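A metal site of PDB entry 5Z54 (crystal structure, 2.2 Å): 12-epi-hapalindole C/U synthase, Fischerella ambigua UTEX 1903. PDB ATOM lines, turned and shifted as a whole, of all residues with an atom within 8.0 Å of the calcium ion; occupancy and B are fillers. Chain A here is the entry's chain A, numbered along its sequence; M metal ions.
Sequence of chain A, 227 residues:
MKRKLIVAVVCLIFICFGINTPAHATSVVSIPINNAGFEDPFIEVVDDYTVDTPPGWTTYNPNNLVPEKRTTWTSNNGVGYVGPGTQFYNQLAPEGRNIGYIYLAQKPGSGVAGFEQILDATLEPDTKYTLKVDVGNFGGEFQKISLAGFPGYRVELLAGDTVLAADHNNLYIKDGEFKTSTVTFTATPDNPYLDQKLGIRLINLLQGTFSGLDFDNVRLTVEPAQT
O of Asp 134 is in hydrogen-bond range of N of Asp 216.
O of Phe 38 lies close to ND2 of Asn 98 (3.2 Å).
N of Arg 97 lies within hydrogen-bond range of OE1 of Glu 39 (2.8 Å).
The backbone NH (N) of Glu 39 lies within hydrogen-bond range of the side-chain amide oxygen (OD1) of Asn 35.
Five residues have an atom within 4 Å of the calcium ion: Gly 37, Glu 39, Glu 95, Asn 98 and Asp 216.
The calcium ion is bound by OE1 of Glu 95 (2.2 Å), O of Asn 98 (2.3 Å), O of Gly 37 (2.3 Å), O of Glu 95 (2.3 Å), OD1 of Asp 216 (2.4 Å), OE2 of Glu 39 (2.4 Å) and OD2 of Asp 216 (2.5 Å).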
ATOM      1  N   ASN A  35     -10.844  24.585   5.596  1.00  0.00           N
ATOM      2  CA  ASN A  35     -12.024  24.946   4.825  1.00  0.00           C
ATOM      3  C   ASN A  35     -12.416  23.736   3.965  1.00  0.00           C
ATOM      4  O   ASN A  35     -12.657  23.855   2.740  1.00  0.00           O
ATOM      5  CB  ASN A  35     -11.798  26.255   4.041  1.00  0.00           C
ATOM      6  CG  ASN A  35     -13.088  26.858   3.494  1.00  0.00           C
ATOM      7  OD1 ASN A  35     -14.191  26.607   4.020  1.00  0.00           O
ATOM      8  ND2 ASN A  35     -12.974  27.589   2.410  1.00  0.00           N
ATOM      9  N   ALA A  36     -12.525  22.586   4.663  1.00  0.00           N
ATOM     10  CA  ALA A  36     -12.592  21.256   4.076  1.00  0.00           C
ATOM     11  C   ALA A  36     -13.957  21.029   3.442  1.00  0.00           C
ATOM     12  O   ALA A  36     -14.134  20.150   2.589  1.00  0.00           O
ATOM     13  CB  ALA A  36     -12.311  20.222   5.158  1.00  0.00           C
ATOM     14  N   GLY A  37     -14.934  21.844   3.862  1.00  0.00           N
ATOM     15  CA  GLY A  37     -16.273  21.723   3.306  1.00  0.00           C
ATOM     16  C   GLY A  37     -16.690  23.015   2.598  1.00  0.00           C
ATOM     17  O   GLY A  37     -17.888  23.212   2.342  1.00  0.00           O
ATOM     18  N   PHE A  38     -15.721  23.880   2.325  1.00  0.00           N
ATOM     19  CA  PHE A  38     -15.905  25.120   1.552  1.00  0.00           C
ATOM     20  C   PHE A  38     -16.892  26.074   2.212  1.00  0.00           C
ATOM     21  O   PHE A  38     -17.505  26.905   1.522  1.00  0.00           O
ATOM     22  CB  PHE A  38     -16.309  24.794   0.102  1.00  0.00           C
ATOM     23  CG  PHE A  38     -15.274  23.957  -0.609  1.00  0.00           C
ATOM     24  CD1 PHE A  38     -14.100  24.538  -1.055  1.00  0.00           C
ATOM     25  CD2 PHE A  38     -15.438  22.594  -0.753  1.00  0.00           C
ATOM     26  CE1 PHE A  38     -13.108  23.779  -1.631  1.00  0.00           C
ATOM     27  CE2 PHE A  38     -14.455  21.826  -1.348  1.00  0.00           C
ATOM     28  CZ  PHE A  38     -13.296  22.426  -1.801  1.00  0.00           C
ATOM     29  N   GLU A  39     -17.029  26.002   3.535  1.00  0.00           N
ATOM     30  CA  GLU A  39     -18.009  26.849   4.264  1.00  0.00           C
ATOM     31  C   GLU A  39     -17.580  28.316   4.287  1.00  0.00           C
ATOM     32  O   GLU A  39     -18.466  29.154   4.368  1.00  0.00           O
ATOM     33  CB  GLU A  39     -18.336  26.248   5.624  1.00  0.00           C
ATOM     34  CG  GLU A  39     -18.983  24.879   5.529  1.00  0.00           C
ATOM     35  CD  GLU A  39     -20.279  24.815   4.738  1.00  0.00           C
ATOM     36  OE1 GLU A  39     -21.211  25.514   5.115  1.00  0.00           O
ATOM     37  OE2 GLU A  39     -20.350  24.063   3.769  1.00  0.00           O
ATOM     38  N   ASP A  40     -16.281  28.594   4.198  1.00  0.00           N
ATOM     39  CA  ASP A  40     -15.772  29.964   4.191  1.00  0.00           C
ATOM     40  C   ASP A  40     -15.576  30.418   2.736  1.00  0.00           C
ATOM     41  O   ASP A  40     -14.878  29.750   1.982  1.00  0.00           O
ATOM     42  CB  ASP A  40     -14.486  30.059   5.016  1.00  0.00           C
ATOM     43  CG  ASP A  40     -13.863  31.463   5.127  1.00  0.00           C
ATOM     44  OD1 ASP A  40     -14.529  32.460   4.729  1.00  0.00           O
ATOM     45  OD2 ASP A  40     -12.700  31.549   5.600  1.00  0.00           O
ATOM     46  N   GLY A  80     -20.142  28.052  -3.665  1.00  0.00           N
ATOM     47  CA  GLY A  80     -21.541  28.281  -4.018  1.00  0.00           C
ATOM     48  C   GLY A  80     -22.455  27.714  -2.934  1.00  0.00           C
ATOM     49  O   GLY A  80     -22.130  26.678  -2.345  1.00  0.00           O
ATOM     50  N   ALA A  93     -26.664  20.697  -0.171  1.00  0.00           N
ATOM     51  CA  ALA A  93     -25.229  20.467  -0.103  1.00  0.00           C
ATOM     52  C   ALA A  93     -24.955  19.226   0.761  1.00  0.00           C
ATOM     53  O   ALA A  93     -25.671  18.965   1.733  1.00  0.00           O
ATOM     54  CB  ALA A  93     -24.505  21.683   0.403  1.00  0.00           C
ATOM     55  N   PRO A  94     -23.990  18.385   0.344  1.00  0.00           N
ATOM     56  CA  PRO A  94     -23.566  17.230   1.125  1.00  0.00           C
ATOM     57  C   PRO A  94     -23.227  17.555   2.590  1.00  0.00           C
ATOM     58  O   PRO A  94     -23.602  16.809   3.477  1.00  0.00           O
ATOM     59  CB  PRO A  94     -22.343  16.730   0.345  1.00  0.00           C
ATOM     60  CG  PRO A  94     -22.675  17.106  -1.093  1.00  0.00           C
ATOM     61  CD  PRO A  94     -23.319  18.467  -0.968  1.00  0.00           C
ATOM     62  N   GLU A  95     -22.616  18.721   2.824  1.00  0.00           N
ATOM     63  CA  GLU A  95     -22.264  19.164   4.186  1.00  0.00           C
ATOM     64  C   GLU A  95     -22.372  20.687   4.292  1.00  0.00           C
ATOM     65  O   GLU A  95     -21.882  21.354   3.388  1.00  0.00           O
ATOM     66  CB  GLU A  95     -20.882  18.657   4.580  1.00  0.00           C
ATOM     67  CG  GLU A  95     -19.778  19.626   4.216  1.00  0.00           C
ATOM     68  CD  GLU A  95     -19.619  20.931   4.997  1.00  0.00           C
ATOM     69  OE1 GLU A  95     -19.069  21.902   4.422  1.00  0.00           O
ATOM     70  OE2 GLU A  95     -20.045  20.994   6.163  1.00  0.00           O
ATOM     71  N   GLY A  96     -22.944  21.172   5.394  1.00  0.00           N
ATOM     72  CA  GLY A  96     -23.181  22.585   5.672  1.00  0.00           C
ATOM     73  C   GLY A  96     -24.003  23.242   4.566  1.00  0.00           C
ATOM     74  O   GLY A  96     -24.939  22.652   4.055  1.00  0.00           O
ATOM     75  N   ARG A  97     -23.583  24.426   4.147  1.00  0.00           N
ATOM     76  CA  ARG A  97     -24.348  25.228   3.214  1.00  0.00           C
ATOM     77  C   ARG A  97     -23.731  25.150   1.820  1.00  0.00           C
ATOM     78  O   ARG A  97     -24.478  25.103   0.842  1.00  0.00           O
ATOM     79  CB  ARG A  97     -24.390  26.688   3.684  1.00  0.00           C
ATOM     80  CG  ARG A  97     -25.331  26.956   4.848  1.00  0.00           C
ATOM     81  CD  ARG A  97     -24.987  28.290   5.484  1.00  0.00           C
ATOM     82  NE  ARG A  97     -25.474  29.383   4.666  1.00  0.00           N
ATOM     83  CZ  ARG A  97     -26.772  29.695   4.517  1.00  0.00           C
ATOM     84  NH1 ARG A  97     -27.694  29.110   5.264  1.00  0.00           N
ATOM     85  NH2 ARG A  97     -27.157  30.583   3.601  1.00  0.00           N
ATOM     86  N   ASN A  98     -22.391  25.096   1.738  1.00  0.00           N
ATOM     87  CA  ASN A  98     -21.653  25.433   0.505  1.00  0.00           C
ATOM     88  C   ASN A  98     -20.946  24.236  -0.144  1.00  0.00           C
ATOM     89  O   ASN A  98     -20.604  23.266   0.524  1.00  0.00           O
ATOM     90  CB  ASN A  98     -20.561  26.425   0.770  1.00  0.00           C
ATOM     91  CG  ASN A  98     -21.084  27.787   1.165  1.00  0.00           C
ATOM     92  OD1 ASN A  98     -22.266  28.086   0.999  1.00  0.00           O
ATOM     93  ND2 ASN A  98     -20.188  28.628   1.647  1.00  0.00           N
ATOM     94  N   ILE A  99     -20.718  24.353  -1.468  1.00  0.00           N
ATOM     95  CA  ILE A  99     -19.891  23.435  -2.203  1.00  0.00           C
ATOM     96  C   ILE A  99     -18.781  24.277  -2.806  1.00  0.00           C
ATOM     97  O   ILE A  99     -18.942  25.476  -2.856  1.00  0.00           O
ATOM     98  CB  ILE A  99     -20.709  22.624  -3.247  1.00  0.00           C
ATOM     99  CG1 ILE A  99     -21.393  23.496  -4.330  1.00  0.00           C
ATOM    100  CG2 ILE A  99     -21.704  21.713  -2.548  1.00  0.00           C
ATOM    101  CD1 ILE A  99     -20.464  24.323  -5.179  1.00  0.00           C
ATOM    102  N   GLY A 100     -17.656  23.650  -3.196  1.00  0.00           N
ATOM    103  CA  GLY A 100     -16.623  24.322  -3.998  1.00  0.00           C
ATOM    104  C   GLY A 100     -16.781  23.930  -5.476  1.00  0.00           C
ATOM    105  O   GLY A 100     -17.127  22.788  -5.750  1.00  0.00           O
ATOM    106  N   ASP A 134     -17.045  14.365  -1.743  1.00  0.00           N
ATOM    107  CA  ASP A 134     -18.270  14.346  -2.520  1.00  0.00           C
ATOM    108  C   ASP A 134     -18.056  15.107  -3.831  1.00  0.00           C
ATOM    109  O   ASP A 134     -17.435  16.164  -3.857  1.00  0.00           O
ATOM    110  CB  ASP A 134     -19.475  14.756  -1.663  1.00  0.00           C
ATOM    111  CG  ASP A 134     -19.601  13.880  -0.414  1.00  0.00           C
ATOM    112  OD1 ASP A 134     -19.601  12.616  -0.564  1.00  0.00           O
ATOM    113  OD2 ASP A 134     -19.666  14.446   0.716  1.00  0.00           O
ATOM    114  N   PHE A 215     -17.430  20.056  -5.541  1.00  0.00           N
ATOM    115  CA  PHE A 215     -16.818  19.185  -4.575  1.00  0.00           C
ATOM    116  C   PHE A 215     -17.309  19.613  -3.205  1.00  0.00           C
ATOM    117  O   PHE A 215     -17.538  20.817  -2.972  1.00  0.00           O
ATOM    118  CB  PHE A 215     -15.314  19.365  -4.651  1.00  0.00           C
ATOM    119  CG  PHE A 215     -14.684  18.815  -5.901  1.00  0.00           C
ATOM    120  CD1 PHE A 215     -14.498  17.449  -6.064  1.00  0.00           C
ATOM    121  CD2 PHE A 215     -14.214  19.684  -6.890  1.00  0.00           C
ATOM    122  CE1 PHE A 215     -13.912  16.952  -7.221  1.00  0.00           C
ATOM    123  CE2 PHE A 215     -13.632  19.178  -8.046  1.00  0.00           C
ATOM    124  CZ  PHE A 215     -13.479  17.817  -8.212  1.00  0.00           C
ATOM    125  N   ASP A 216     -17.485  18.638  -2.295  1.00  0.00           N
ATOM    126  CA  ASP A 216     -17.727  19.003  -0.900  1.00  0.00           C
ATOM    127  C   ASP A 216     -17.049  18.022   0.050  1.00  0.00           C
ATOM    128  O   ASP A 216     -16.619  16.928  -0.341  1.00  0.00           O
ATOM    129  CB  ASP A 216     -19.218  19.098  -0.577  1.00  0.00           C
ATOM    130  CG  ASP A 216     -19.515  20.007   0.631  1.00  0.00           C
ATOM    131  OD1 ASP A 216     -18.573  20.556   1.212  1.00  0.00           O
ATOM    132  OD2 ASP A 216     -20.670  20.196   0.960  1.00  0.00           O
ATOM    133  N   ASN A 217     -16.969  18.452   1.309  1.00  0.00           N
ATOM    134  CA  ASN A 217     -16.797  17.565   2.438  1.00  0.00           C
ATOM    135  C   ASN A 217     -15.569  16.685   2.247  1.00  0.00           C
ATOM    136  O   ASN A 217     -15.696  15.470   2.086  1.00  0.00           O
ATOM    137  CB  ASN A 217     -17.970  16.607   2.582  1.00  0.00           C
ATOM    138  CG  ASN A 217     -18.002  16.011   3.967  1.00  0.00           C
ATOM    139  OD1 ASN A 217     -17.289  16.479   4.866  1.00  0.00           O
ATOM    140  ND2 ASN A 217     -18.782  14.978   4.142  1.00  0.00           N
ATOM    141  N   VAL A 218     -14.414  17.318   2.237  1.00  0.00           N
ATOM    142  CA  VAL A 218     -13.166  16.636   2.003  1.00  0.00           C
ATOM    143  C   VAL A 218     -12.672  16.140   3.361  1.00  0.00           C
ATOM    144  O   VAL A 218     -12.558  16.924   4.299  1.00  0.00           O
ATOM    145  CB  VAL A 218     -12.179  17.613   1.368  1.00  0.00           C
ATOM    146  CG1 VAL A 218     -10.839  16.955   1.032  1.00  0.00           C
ATOM    147  CG2 VAL A 218     -12.788  18.255   0.131  1.00  0.00           C
HETATM  148 CA    CA M   1     -19.921  22.115   2.394  1.00  0.00          CA
